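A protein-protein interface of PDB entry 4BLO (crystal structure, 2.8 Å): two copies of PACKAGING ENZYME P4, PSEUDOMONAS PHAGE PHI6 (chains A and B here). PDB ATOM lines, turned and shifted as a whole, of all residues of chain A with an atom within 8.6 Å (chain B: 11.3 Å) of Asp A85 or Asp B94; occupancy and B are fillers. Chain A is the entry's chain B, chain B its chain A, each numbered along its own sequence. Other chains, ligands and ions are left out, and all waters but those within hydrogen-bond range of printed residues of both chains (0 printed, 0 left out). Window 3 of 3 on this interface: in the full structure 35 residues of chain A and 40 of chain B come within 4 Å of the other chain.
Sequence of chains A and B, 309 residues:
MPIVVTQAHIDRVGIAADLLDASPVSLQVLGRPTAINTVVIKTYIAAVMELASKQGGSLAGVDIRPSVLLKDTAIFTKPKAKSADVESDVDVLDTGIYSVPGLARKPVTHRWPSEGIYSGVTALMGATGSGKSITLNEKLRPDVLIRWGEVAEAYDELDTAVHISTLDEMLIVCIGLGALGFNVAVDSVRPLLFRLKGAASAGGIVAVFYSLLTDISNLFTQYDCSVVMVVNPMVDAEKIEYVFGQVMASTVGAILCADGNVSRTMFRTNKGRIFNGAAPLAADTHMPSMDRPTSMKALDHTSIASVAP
Printed residues of chain B within 4 Å of Leu A30: Asp B91 (3.4 Å). Of the printed residues of chain B, Gly A31 touches Asp B91 (3.4 Å). Of the printed residues of chain B, Thr A34 touches Leu B93. Asp A85 touches just these residues of chain B: Arg B32 (3.1 Å) and Asp B94 (3.8 Å). Of chain B, only Val B90 (3.5 Å), Asp B91 (2.9 Å) and Asp B94 (2.8 Å) come within 4 Å of Val A86. Of the printed residues of chain A, Leu B30 touches Lys A197. Gly B31 touches none of the printed residues of chain A. Of the printed residues of chain A, Val B92 touches Val A29 and Lys A197. Asp B94 touches two residues of chain A. Thr B95 touches none of the printed residues of chain A. Tyr B98 touches none of the printed residues of chain A. The nearest printed residue of chain A that does not touch Val B90 is Glu A87 (4.03 Å).
The backbone carbonyl oxygen (O) of Leu A27 sits at hydrogen-bond distance from the backbone NH (N) of Thr A34 (2.7 Å). The backbone carbonyl oxygen of Gly A31 sits at hydrogen-bond distance from the side-chain amide nitrogen of Gln A28 (2.8 Å). The side-chain hydroxyl of Thr A95 sits close to the backbone carbonyl oxygen of Gly A31 (3.4 Å). O of Arg A32 lies within hydrogen-bond range of OG1 of Thr A34, at 3.3 Å.
NH1 of Arg B32 lies within salt-bridge range of OD1 of Asp A85 (3.1 Å). The backbone carbonyl oxygen (O) of Ser B88 lies within hydrogen-bond range of the side-chain amino group (NZ) of Lys A197 (2.9 Å). The side-chain hydroxyl of Ser A88 sits at hydrogen-bond distance from the backbone carbonyl oxygen of Val B90, 3.4 Å away. The backbone carbonyl oxygen (O) of Val B90 sits at hydrogen-bond distance from the side-chain amino group (NZ) of Lys A197. OD1 of Asp B91 is in hydrogen-bond range of N of Leu A30, at 3.4 Å. The side-chain carboxylate of Asp B91 sits close to the backbone NH of Gly A31. O of Val A86 lies within hydrogen-bond range of N of Asp B91. The backbone NH (N) of Val A86 sits at hydrogen-bond distance from the side-chain carboxylate (OD2) of Asp B94, at 2.8 Å. OE1 of Glu A87 lies close to O of Asp B89 (3.3 Å). NZ of Lys A197 sits close to O of Leu B30, at 2.2 Å.
Asp A85 touches Arg B32, but with the chains exchanged Arg A32 does not touch Asp B85 (15.3 Å). Val A86 touches Val B90, but with the chains exchanged Val A90 does not touch Val B86 (13.2 Å). Glu B87 touches its own counterpart, Glu A87. Ser A88 touches Val B90, but with the chains exchanged Val A90 does not touch Ser B88 (11.7 Å).
Among the printed residues, pairs that only touch across the chains: Leu A27 with Leu B93, Gln A28 with Leu B93, Val A29 with Asp B91, Val A29 with Val B92, Val A29 with Leu B93, Arg A32 with Asp B91, Thr A34 with Leu B93, Asp A85 with Asp B94, Val A86 with Val B90, Glu A87 with Glu B87, Ser A88 with Asp B89, Ser A88 with Asp B91, Leu A167 with Ile B97, Lys A197 with Asp B89 and Lys A197 with Val B92.
Hydrophobic or aromatic side chains of chain B within 4 Å of the printed part of chain A: Val B90, Val B92, Leu B93 and Ile B97. Of the 19 printed residues of chain A, 13 touch a printed residue of chain B. Hydrophobic or aromatic side chains of chain A that line the printed part of chain B: Val A29, Val A86 and Leu A167. Among the printed residues, 25 pairs touch across the chains.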
ATOM      1  N   LEU A  27     -27.882  13.027 -16.649  1.00  0.00           N
ATOM      2  CA  LEU A  27     -27.523  13.094 -18.058  1.00  0.00           C
ATOM      3  C   LEU A  27     -27.734  11.733 -18.679  1.00  0.00           C
ATOM      4  O   LEU A  27     -27.617  10.714 -17.997  1.00  0.00           O
ATOM      5  CB  LEU A  27     -26.087  13.595 -18.277  1.00  0.00           C
ATOM      6  CG  LEU A  27     -25.805  14.234 -19.644  1.00  0.00           C
ATOM      7  CD1 LEU A  27     -26.320  15.670 -19.716  1.00  0.00           C
ATOM      8  CD2 LEU A  27     -24.344  14.198 -19.946  1.00  0.00           C
ATOM      9  N   GLN A  28     -28.120  11.677 -19.939  1.00  0.00           N
ATOM     10  CA  GLN A  28     -28.335  10.445 -20.668  1.00  0.00           C
ATOM     11  C   GLN A  28     -27.838  10.607 -22.096  1.00  0.00           C
ATOM     12  O   GLN A  28     -27.982  11.692 -22.682  1.00  0.00           O
ATOM     13  CB  GLN A  28     -29.810  10.050 -20.648  1.00  0.00           C
ATOM     14  CG  GLN A  28     -30.066   8.592 -21.037  1.00  0.00           C
ATOM     15  CD  GLN A  28     -31.475   8.345 -21.514  1.00  0.00           C
ATOM     16  OE1 GLN A  28     -32.238   9.262 -21.819  1.00  0.00           O
ATOM     17  NE2 GLN A  28     -31.852   7.097 -21.591  1.00  0.00           N
ATOM     18  N   VAL A  29     -27.250   9.538 -22.624  1.00  0.00           N
ATOM     19  CA  VAL A  29     -26.922   9.429 -24.037  1.00  0.00           C
ATOM     20  C   VAL A  29     -27.428   8.488 -25.138  1.00  0.00           C
ATOM     21  O   VAL A  29     -28.062   8.933 -26.094  1.00  0.00           O
ATOM     22  CB  VAL A  29     -25.418   9.160 -24.254  1.00  0.00           C
ATOM     23  CG1 VAL A  29     -25.041   9.400 -25.707  1.00  0.00           C
ATOM     24  CG2 VAL A  29     -24.585  10.033 -23.328  1.00  0.00           C
ATOM     25  N   LEU A  30     -27.153   7.192 -25.001  1.00  0.00           N
ATOM     26  CA  LEU A  30     -27.868   6.043 -25.552  1.00  0.00           C
ATOM     27  C   LEU A  30     -28.147   4.942 -24.523  1.00  0.00           C
ATOM     28  O   LEU A  30     -28.699   3.896 -24.864  1.00  0.00           O
ATOM     29  CB  LEU A  30     -27.102   5.461 -26.743  1.00  0.00           C
ATOM     30  CG  LEU A  30     -27.130   6.283 -28.033  1.00  0.00           C
ATOM     31  CD1 LEU A  30     -26.549   5.485 -29.191  1.00  0.00           C
ATOM     32  CD2 LEU A  30     -28.546   6.740 -28.350  1.00  0.00           C
ATOM     33  N   GLY A  31     -27.758   5.173 -23.273  1.00  0.00           N
ATOM     34  CA  GLY A  31     -27.858   4.156 -22.242  1.00  0.00           C
ATOM     35  C   GLY A  31     -28.931   4.533 -21.247  1.00  0.00           C
ATOM     36  O   GLY A  31     -30.046   4.899 -21.640  1.00  0.00           O
ATOM     37  N   ARG A  32     -28.616   4.496 -19.984  1.00  0.00           N
ATOM     38  CA  ARG A  32     -29.574   4.879 -18.955  1.00  0.00           C
ATOM     39  C   ARG A  32     -29.198   6.234 -18.306  1.00  0.00           C
ATOM     40  O   ARG A  32     -28.017   6.625 -18.332  1.00  0.00           O
ATOM     41  CB  ARG A  32     -29.780   3.775 -17.902  1.00  0.00           C
ATOM     42  CG  ARG A  32     -28.546   3.161 -17.237  1.00  0.00           C
ATOM     43  CD  ARG A  32     -28.753   1.660 -16.983  1.00  0.00           C
ATOM     44  NE  ARG A  32     -29.978   1.346 -16.232  1.00  0.00           N
ATOM     45  CZ  ARG A  32     -30.943   0.528 -16.652  1.00  0.00           C
ATOM     46  NH1 ARG A  32     -30.840  -0.085 -17.827  1.00  0.00           N
ATOM     47  NH2 ARG A  32     -32.012   0.311 -15.898  1.00  0.00           N
ATOM     48  N   PRO A  33     -30.189   7.008 -17.805  1.00  0.00           N
ATOM     49  CA  PRO A  33     -29.859   8.297 -17.180  1.00  0.00           C
ATOM     50  C   PRO A  33     -28.925   8.118 -15.975  1.00  0.00           C
ATOM     51  O   PRO A  33     -29.121   7.212 -15.155  1.00  0.00           O
ATOM     52  CB  PRO A  33     -31.227   8.854 -16.767  1.00  0.00           C
ATOM     53  CG  PRO A  33     -32.212   8.107 -17.586  1.00  0.00           C
ATOM     54  CD  PRO A  33     -31.641   6.747 -17.734  1.00  0.00           C
ATOM     55  N   THR A  34     -27.885   8.947 -15.907  1.00  0.00           N
ATOM     56  CA  THR A  34     -26.898   8.918 -14.837  1.00  0.00           C
ATOM     57  C   THR A  34     -26.910  10.256 -14.098  1.00  0.00           C
ATOM     58  O   THR A  34     -26.764  11.307 -14.719  1.00  0.00           O
ATOM     59  CB  THR A  34     -25.487   8.578 -15.383  1.00  0.00           C
ATOM     60  OG1 THR A  34     -25.588   7.541 -16.375  1.00  0.00           O
ATOM     61  CG2 THR A  34     -24.530   8.145 -14.277  1.00  0.00           C
ATOM     62  N   PHE A  76     -20.365  11.519 -12.301  1.00  0.00           N
ATOM     63  CA  PHE A  76     -21.450  10.584 -12.586  1.00  0.00           C
ATOM     64  C   PHE A  76     -21.421   9.422 -11.593  1.00  0.00           C
ATOM     65  O   PHE A  76     -20.373   8.786 -11.411  1.00  0.00           O
ATOM     66  CB  PHE A  76     -21.374  10.084 -14.037  1.00  0.00           C
ATOM     67  CG  PHE A  76     -21.556  11.160 -15.078  1.00  0.00           C
ATOM     68  CD1 PHE A  76     -22.779  11.801 -15.235  1.00  0.00           C
ATOM     69  CD2 PHE A  76     -20.516  11.504 -15.934  1.00  0.00           C
ATOM     70  CE1 PHE A  76     -22.941  12.800 -16.201  1.00  0.00           C
ATOM     71  CE2 PHE A  76     -20.673  12.512 -16.895  1.00  0.00           C
ATOM     72  CZ  PHE A  76     -21.885  13.152 -17.024  1.00  0.00           C
ATOM     73  N   THR A  77     -22.581   9.165 -10.942  1.00  0.00           N
ATOM     74  CA  THR A  77     -22.746   8.131  -9.916  1.00  0.00           C
ATOM     75  C   THR A  77     -23.812   7.124 -10.340  1.00  0.00           C
ATOM     76  O   THR A  77     -24.935   7.512 -10.656  1.00  0.00           O
ATOM     77  CB  THR A  77     -23.086   8.775  -8.548  1.00  0.00           C
ATOM     78  OG1 THR A  77     -24.236   9.612  -8.693  1.00  0.00           O
ATOM     79  CG2 THR A  77     -21.916   9.571  -7.961  1.00  0.00           C
ATOM     80  N   ALA A  84     -25.356  -3.291 -14.403  1.00  0.00           N
ATOM     81  CA  ALA A  84     -24.056  -2.686 -14.157  1.00  0.00           C
ATOM     82  C   ALA A  84     -23.643  -1.796 -15.339  1.00  0.00           C
ATOM     83  O   ALA A  84     -23.486  -0.585 -15.154  1.00  0.00           O
ATOM     84  CB  ALA A  84     -23.014  -3.770 -13.900  1.00  0.00           C
ATOM     85  N   ASP A  85     -23.486  -2.386 -16.552  1.00  0.00           N
ATOM     86  CA  ASP A  85     -23.100  -1.672 -17.780  1.00  0.00           C
ATOM     87  C   ASP A  85     -24.171  -1.876 -18.854  1.00  0.00           C
ATOM     88  O   ASP A  85     -24.526  -3.022 -19.148  1.00  0.00           O
ATOM     89  CB  ASP A  85     -21.704  -2.122 -18.282  1.00  0.00           C
ATOM     90  CG  ASP A  85     -20.540  -1.574 -17.469  1.00  0.00           C
ATOM     91  OD1 ASP A  85     -20.256  -0.358 -17.577  1.00  0.00           O
ATOM     92  OD2 ASP A  85     -19.900  -2.365 -16.740  1.00  0.00           O
ATOM     93  N   VAL A  86     -24.703  -0.764 -19.416  1.00  0.00           N
ATOM     94  CA  VAL A  86     -25.765  -0.798 -20.421  1.00  0.00           C
ATOM     95  C   VAL A  86     -25.207  -0.471 -21.832  1.00  0.00           C
ATOM     96  O   VAL A  86     -24.348   0.398 -21.987  1.00  0.00           O
ATOM     97  CB  VAL A  86     -26.991   0.090 -20.020  1.00  0.00           C
ATOM     98  CG1 VAL A  86     -26.711   1.569 -20.171  1.00  0.00           C
ATOM     99  CG2 VAL A  86     -28.248  -0.287 -20.793  1.00  0.00           C
ATOM    100  N   GLU A  87     -25.703  -1.210 -22.845  1.00  0.00           N
ATOM    101  CA  GLU A  87     -25.348  -1.079 -24.260  1.00  0.00           C
ATOM    102  C   GLU A  87     -26.065   0.115 -24.899  1.00  0.00           C
ATOM    103  O   GLU A  87     -27.147   0.476 -24.456  1.00  0.00           O
ATOM    104  CB  GLU A  87     -25.735  -2.357 -25.017  1.00  0.00           C
ATOM    105  CG  GLU A  87     -25.101  -3.635 -24.489  1.00  0.00           C
ATOM    106  CD  GLU A  87     -23.860  -4.092 -25.224  1.00  0.00           C
ATOM    107  OE1 GLU A  87     -23.955  -4.376 -26.441  1.00  0.00           O
ATOM    108  OE2 GLU A  87     -22.802  -4.235 -24.567  1.00  0.00           O
ATOM    109  N   SER A  88     -25.495   0.693 -25.967  1.00  0.00           N
ATOM    110  CA  SER A  88     -26.112   1.803 -26.697  1.00  0.00           C
ATOM    111  C   SER A  88     -27.367   1.345 -27.503  1.00  0.00           C
ATOM    112  O   SER A  88     -28.140   2.185 -27.947  1.00  0.00           O
ATOM    113  CB  SER A  88     -25.093   2.449 -27.632  1.00  0.00           C
ATOM    114  OG  SER A  88     -23.977   2.987 -26.946  1.00  0.00           O
ATOM    115  N   VAL A  90     -30.212  -0.685 -26.511  1.00  0.00           N
ATOM    116  CA  VAL A  90     -31.064  -1.227 -25.447  1.00  0.00           C
ATOM    117  C   VAL A  90     -32.438  -0.543 -25.594  1.00  0.00           C
ATOM    118  O   VAL A  90     -32.481   0.606 -26.031  1.00  0.00           O
ATOM    119  CB  VAL A  90     -30.402  -0.985 -24.054  1.00  0.00           C
ATOM    120  CG1 VAL A  90     -30.269   0.503 -23.757  1.00  0.00           C
ATOM    121  CG2 VAL A  90     -31.148  -1.695 -22.927  1.00  0.00           C
ATOM    122  N   THR A  95     -34.736   1.777 -20.234  1.00  0.00           N
ATOM    123  CA  THR A  95     -33.818   2.739 -19.634  1.00  0.00           C
ATOM    124  C   THR A  95     -34.554   4.015 -19.232  1.00  0.00           C
ATOM    125  O   THR A  95     -34.149   4.700 -18.286  1.00  0.00           O
ATOM    126  CB  THR A  95     -32.667   3.075 -20.596  1.00  0.00           C
ATOM    127  OG1 THR A  95     -33.163   3.596 -21.839  1.00  0.00           O
ATOM    128  CG2 THR A  95     -31.748   1.894 -20.829  1.00  0.00           C
ATOM    129  N   LEU A 167     -14.645  13.562 -19.192  1.00  0.00           N
ATOM    130  CA  LEU A 167     -15.869  14.356 -19.373  1.00  0.00           C
ATOM    131  C   LEU A 167     -16.317  14.919 -18.018  1.00  0.00           C
ATOM    132  O   LEU A 167     -16.809  16.055 -17.960  1.00  0.00           O
ATOM    133  CB  LEU A 167     -16.987  13.499 -20.019  1.00  0.00           C
ATOM    134  CG  LEU A 167     -18.380  14.148 -20.155  1.00  0.00           C
ATOM    135  CD1 LEU A 167     -18.348  15.372 -21.083  1.00  0.00           C
ATOM    136  CD2 LEU A 167     -19.440  13.123 -20.573  1.00  0.00           C
ATOM    137  N   LYS A 197     -21.294   6.370 -29.992  1.00  0.00           N
ATOM    138  CA  LYS A 197     -21.675   5.129 -30.680  1.00  0.00           C
ATOM    139  C   LYS A 197     -23.140   5.202 -31.001  1.00  0.00           C
ATOM    140  O   LYS A 197     -23.904   5.754 -30.214  1.00  0.00           O
ATOM    141  CB  LYS A 197     -21.367   3.881 -29.827  1.00  0.00           C
ATOM    142  CG  LYS A 197     -20.795   4.159 -28.435  1.00  0.00           C
ATOM    143  CD  LYS A 197     -19.432   3.512 -28.293  1.00  0.00           C
ATOM    144  CE  LYS A 197     -18.742   3.720 -27.005  1.00  0.00           C
ATOM    145  NZ  LYS A 197     -18.312   2.385 -26.551  1.00  0.00           N
ATOM    146  N   GLN B  28      -7.958   5.076 -24.160  1.00  0.00           N
ATOM    147  CA  GLN B  28      -9.307   4.621 -24.417  1.00  0.00           C
ATOM    148  C   GLN B  28      -9.561   4.605 -25.915  1.00  0.00           C
ATOM    149  O   GLN B  28      -9.071   5.490 -26.636  1.00  0.00           O
ATOM    150  CB  GLN B  28     -10.326   5.505 -23.702  1.00  0.00           C
ATOM    151  CG  GLN B  28     -11.719   4.880 -23.589  1.00  0.00           C
ATOM    152  CD  GLN B  28     -12.810   5.898 -23.375  1.00  0.00           C
ATOM    153  OE1 GLN B  28     -12.632   7.102 -23.555  1.00  0.00           O
ATOM    154  NE2 GLN B  28     -13.969   5.435 -22.988  1.00  0.00           N
ATOM    155  N   LEU B  30     -13.051   2.524 -27.927  1.00  0.00           N
ATOM    156  CA  LEU B  30     -14.509   2.468 -27.844  1.00  0.00           C
ATOM    157  C   LEU B  30     -15.028   1.814 -26.558  1.00  0.00           C
ATOM    158  O   LEU B  30     -16.235   1.660 -26.381  1.00  0.00           O
ATOM    159  CB  LEU B  30     -15.085   1.746 -29.064  1.00  0.00           C
ATOM    160  CG  LEU B  30     -15.044   2.512 -30.388  1.00  0.00           C
ATOM    161  CD1 LEU B  30     -15.859   1.791 -31.451  1.00  0.00           C
ATOM    162  CD2 LEU B  30     -15.540   3.937 -30.201  1.00  0.00           C
ATOM    163  N   GLY B  31     -14.117   1.426 -25.671  1.00  0.00           N
ATOM    164  CA  GLY B  31     -14.482   0.687 -24.477  1.00  0.00           C
ATOM    165  C   GLY B  31     -14.297   1.556 -23.255  1.00  0.00           C
ATOM    166  O   GLY B  31     -14.746   2.710 -23.235  1.00  0.00           O
ATOM    167  N   ARG B  32     -13.623   1.021 -22.228  1.00  0.00           N
ATOM    168  CA  ARG B  32     -13.382   1.811 -21.024  1.00  0.00           C
ATOM    169  C   ARG B  32     -11.902   2.246 -20.934  1.00  0.00           C
ATOM    170  O   ARG B  32     -11.033   1.588 -21.521  1.00  0.00           O
ATOM    171  CB  ARG B  32     -13.864   1.102 -19.744  1.00  0.00           C
ATOM    172  CG  ARG B  32     -13.434  -0.335 -19.503  1.00  0.00           C
ATOM    173  CD  ARG B  32     -14.569  -1.145 -18.858  1.00  0.00           C
ATOM    174  NE  ARG B  32     -15.104  -0.552 -17.623  1.00  0.00           N
ATOM    175  CZ  ARG B  32     -16.389  -0.263 -17.414  1.00  0.00           C
ATOM    176  NH1 ARG B  32     -17.295  -0.505 -18.354  1.00  0.00           N
ATOM    177  NH2 ARG B  32     -16.776   0.268 -16.261  1.00  0.00           N
ATOM    178  N   PRO B  33     -11.603   3.395 -20.280  1.00  0.00           N
ATOM    179  CA  PRO B  33     -10.189   3.825 -20.168  1.00  0.00           C
ATOM    180  C   PRO B  33      -9.323   2.802 -19.427  1.00  0.00           C
ATOM    181  O   PRO B  33      -9.728   2.269 -18.386  1.00  0.00           O
ATOM    182  CB  PRO B  33     -10.282   5.142 -19.387  1.00  0.00           C
ATOM    183  CG  PRO B  33     -11.716   5.572 -19.511  1.00  0.00           C
ATOM    184  CD  PRO B  33     -12.505   4.323 -19.559  1.00  0.00           C
ATOM    185  N   ALA B  84     -15.526  -7.311 -16.735  1.00  0.00           N
ATOM    186  CA  ALA B  84     -14.253  -7.887 -17.148  1.00  0.00           C
ATOM    187  C   ALA B  84     -13.877  -7.405 -18.561  1.00  0.00           C
ATOM    188  O   ALA B  84     -12.867  -6.710 -18.718  1.00  0.00           O
ATOM    189  CB  ALA B  84     -14.323  -9.411 -17.093  1.00  0.00           C
ATOM    190  N   ASP B  85     -14.705  -7.741 -19.576  1.00  0.00           N
ATOM    191  CA  ASP B  85     -14.485  -7.346 -20.973  1.00  0.00           C
ATOM    192  C   ASP B  85     -15.674  -6.499 -21.472  1.00  0.00           C
ATOM    193  O   ASP B  85     -16.825  -6.909 -21.320  1.00  0.00           O
ATOM    194  CB  ASP B  85     -14.234  -8.573 -21.873  1.00  0.00           C
ATOM    195  CG  ASP B  85     -12.845  -9.187 -21.723  1.00  0.00           C
ATOM    196  OD1 ASP B  85     -11.867  -8.574 -22.207  1.00  0.00           O
ATOM    197  OD2 ASP B  85     -12.741 -10.292 -21.148  1.00  0.00           O
ATOM    198  N   VAL B  86     -15.385  -5.302 -22.029  1.00  0.00           N
ATOM    199  CA  VAL B  86     -16.395  -4.350 -22.491  1.00  0.00           C
ATOM    200  C   VAL B  86     -16.504  -4.348 -24.042  1.00  0.00           C
ATOM    201  O   VAL B  86     -15.506  -4.476 -24.755  1.00  0.00           O
ATOM    202  CB  VAL B  86     -16.144  -2.930 -21.886  1.00  0.00           C
ATOM    203  CG1 VAL B  86     -14.935  -2.234 -22.495  1.00  0.00           C
ATOM    204  CG2 VAL B  86     -17.383  -2.052 -21.974  1.00  0.00           C
ATOM    205  N   GLU B  87     -17.747  -4.223 -24.536  1.00  0.00           N
ATOM    206  CA  GLU B  87     -18.106  -4.178 -25.958  1.00  0.00           C
ATOM    207  C   GLU B  87     -17.834  -2.790 -26.539  1.00  0.00           C
ATOM    208  O   GLU B  87     -17.911  -1.810 -25.803  1.00  0.00           O
ATOM    209  CB  GLU B  87     -19.600  -4.527 -26.132  1.00  0.00           C
ATOM    210  CG  GLU B  87     -19.983  -5.917 -25.652  1.00  0.00           C
ATOM    211  CD  GLU B  87     -19.981  -7.024 -26.692  1.00  0.00           C
ATOM    212  OE1 GLU B  87     -20.704  -6.905 -27.707  1.00  0.00           O
ATOM    213  OE2 GLU B  87     -19.307  -8.049 -26.449  1.00  0.00           O
ATOM    214  N   SER B  88     -17.572  -2.692 -27.856  1.00  0.00           N
ATOM    215  CA  SER B  88     -17.353  -1.402 -28.519  1.00  0.00           C
ATOM    216  C   SER B  88     -18.664  -0.564 -28.598  1.00  0.00           C
ATOM    217  O   SER B  88     -18.600   0.635 -28.863  1.00  0.00           O
ATOM    218  CB  SER B  88     -16.774  -1.605 -29.919  1.00  0.00           C
ATOM    219  OG  SER B  88     -15.495  -2.212 -29.897  1.00  0.00           O
ATOM    220  N   ASP B  89     -19.838  -1.189 -28.376  1.00  0.00           N
ATOM    221  CA  ASP B  89     -21.132  -0.503 -28.417  1.00  0.00           C
ATOM    222  C   ASP B  89     -21.775  -0.600 -27.036  1.00  0.00           C
ATOM    223  O   ASP B  89     -22.698  -1.395 -26.810  1.00  0.00           O
ATOM    224  CB  ASP B  89     -22.054  -1.058 -29.532  1.00  0.00           C
ATOM    225  CG  ASP B  89     -21.615  -0.784 -30.965  1.00  0.00           C
ATOM    226  OD1 ASP B  89     -20.877   0.203 -31.186  1.00  0.00           O
ATOM    227  OD2 ASP B  89     -22.009  -1.565 -31.868  1.00  0.00           O
ATOM    228  N   VAL B  90     -21.223   0.185 -26.108  1.00  0.00           N
ATOM    229  CA  VAL B  90     -21.600   0.328 -24.699  1.00  0.00           C
ATOM    230  C   VAL B  90     -21.822   1.834 -24.448  1.00  0.00           C
ATOM    231  O   VAL B  90     -21.133   2.644 -25.078  1.00  0.00           O
ATOM    232  CB  VAL B  90     -20.491  -0.284 -23.786  1.00  0.00           C
ATOM    233  CG1 VAL B  90     -19.162   0.468 -23.926  1.00  0.00           C
ATOM    234  CG2 VAL B  90     -20.927  -0.345 -22.320  1.00  0.00           C
ATOM    235  N   ASP B  91     -22.746   2.225 -23.549  1.00  0.00           N
ATOM    236  CA  ASP B  91     -22.995   3.649 -23.317  1.00  0.00           C
ATOM    237  C   ASP B  91     -21.732   4.382 -22.801  1.00  0.00           C
ATOM    238  O   ASP B  91     -21.102   3.978 -21.817  1.00  0.00           O
ATOM    239  CB  ASP B  91     -24.175   3.873 -22.364  1.00  0.00           C
ATOM    240  CG  ASP B  91     -24.558   5.332 -22.212  1.00  0.00           C
ATOM    241  OD1 ASP B  91     -24.470   6.077 -23.208  1.00  0.00           O
ATOM    242  OD2 ASP B  91     -25.028   5.707 -21.124  1.00  0.00           O
ATOM    243  N   VAL B  92     -21.393   5.473 -23.502  1.00  0.00           N
ATOM    244  CA  VAL B  92     -20.253   6.374 -23.270  1.00  0.00           C
ATOM    245  C   VAL B  92     -20.281   6.956 -21.854  1.00  0.00           C
ATOM    246  O   VAL B  92     -19.239   7.313 -21.317  1.00  0.00           O
ATOM    247  CB  VAL B  92     -20.213   7.519 -24.323  1.00  0.00           C
ATOM    248  CG1 VAL B  92     -19.856   7.014 -25.705  1.00  0.00           C
ATOM    249  CG2 VAL B  92     -21.501   8.331 -24.355  1.00  0.00           C
ATOM    250  N   LEU B  93     -21.471   7.052 -21.255  1.00  0.00           N
ATOM    251  CA  LEU B  93     -21.677   7.551 -19.902  1.00  0.00           C
ATOM    252  C   LEU B  93     -21.366   6.480 -18.848  1.00  0.00           C
ATOM    253  O   LEU B  93     -21.073   6.834 -17.710  1.00  0.00           O
ATOM    254  CB  LEU B  93     -23.130   8.030 -19.763  1.00  0.00           C
ATOM    255  CG  LEU B  93     -23.367   9.419 -19.197  1.00  0.00           C
ATOM    256  CD1 LEU B  93     -22.689  10.507 -20.022  1.00  0.00           C
ATOM    257  CD2 LEU B  93     -24.814   9.699 -19.124  1.00  0.00           C
ATOM    258  N   ASP B  94     -21.450   5.183 -19.217  1.00  0.00           N
ATOM    259  CA  ASP B  94     -21.160   4.061 -18.317  1.00  0.00           C
ATOM    260  C   ASP B  94     -19.656   3.751 -18.254  1.00  0.00           C
ATOM    261  O   ASP B  94     -19.185   3.240 -17.233  1.00  0.00           O
ATOM    262  CB  ASP B  94     -21.935   2.801 -18.728  1.00  0.00           C
ATOM    263  CG  ASP B  94     -23.430   2.797 -18.438  1.00  0.00           C
ATOM    264  OD1 ASP B  94     -23.917   3.718 -17.731  1.00  0.00           O
ATOM    265  OD2 ASP B  94     -24.110   1.877 -18.900  1.00  0.00           O
ATOM    266  N   THR B  95     -18.908   4.060 -19.334  1.00  0.00           N
ATOM    267  CA  THR B  95     -17.463   3.836 -19.404  1.00  0.00           C
ATOM    268  C   THR B  95     -16.706   5.100 -19.061  1.00  0.00           C
ATOM    269  O   THR B  95     -15.589   5.036 -18.536  1.00  0.00           O
ATOM    270  CB  THR B  95     -17.041   3.334 -20.796  1.00  0.00           C
ATOM    271  OG1 THR B  95     -17.434   4.262 -21.817  1.00  0.00           O
ATOM    272  CG2 THR B  95     -17.566   1.949 -21.098  1.00  0.00           C
ATOM    273  N   GLY B  96     -17.317   6.238 -19.382  1.00  0.00           N
ATOM    274  CA  GLY B  96     -16.708   7.550 -19.237  1.00  0.00           C
ATOM    275  C   GLY B  96     -15.857   7.821 -20.467  1.00  0.00           C
ATOM    276  O   GLY B  96     -15.758   6.957 -21.343  1.00  0.00           O
ATOM    277  N   ILE B  97     -15.245   9.014 -20.556  1.00  0.00           N
ATOM    278  CA  ILE B  97     -14.394   9.377 -21.696  1.00  0.00           C
ATOM    279  C   ILE B  97     -13.041   9.820 -21.176  1.00  0.00           C
ATOM    280  O   ILE B  97     -12.988  10.591 -20.233  1.00  0.00           O
ATOM    281  CB  ILE B  97     -15.046  10.451 -22.619  1.00  0.00           C
ATOM    282  CG1 ILE B  97     -16.320   9.930 -23.267  1.00  0.00           C
ATOM    283  CG2 ILE B  97     -14.086  10.954 -23.698  1.00  0.00           C
ATOM    284  CD1 ILE B  97     -17.389  10.852 -23.136  1.00  0.00           C
ATOM    285  N   TYR B  98     -11.957   9.334 -21.787  1.00  0.00           N
ATOM    286  CA  TYR B  98     -10.604   9.701 -21.425  1.00  0.00           C
ATOM    287  C   TYR B  98      -9.791  10.101 -22.650  1.00  0.00           C
ATOM    288  O   TYR B  98      -9.786   9.398 -23.671  1.00  0.00           O
ATOM    289  CB  TYR B  98      -9.887   8.560 -20.683  1.00  0.00           C
ATOM    290  CG  TYR B  98      -8.479   8.909 -20.233  1.00  0.00           C
ATOM    291  CD1 TYR B  98      -7.395   8.792 -21.103  1.00  0.00           C
ATOM    292  CD2 TYR B  98      -8.230   9.352 -18.939  1.00  0.00           C
ATOM    293  CE1 TYR B  98      -6.111   9.153 -20.712  1.00  0.00           C
ATOM    294  CE2 TYR B  98      -6.939   9.670 -18.521  1.00  0.00           C
ATOM    295  CZ  TYR B  98      -5.884   9.582 -19.417  1.00  0.00           C
ATOM    296  OH  TYR B  98      -4.610   9.908 -19.037  1.00  0.00           O
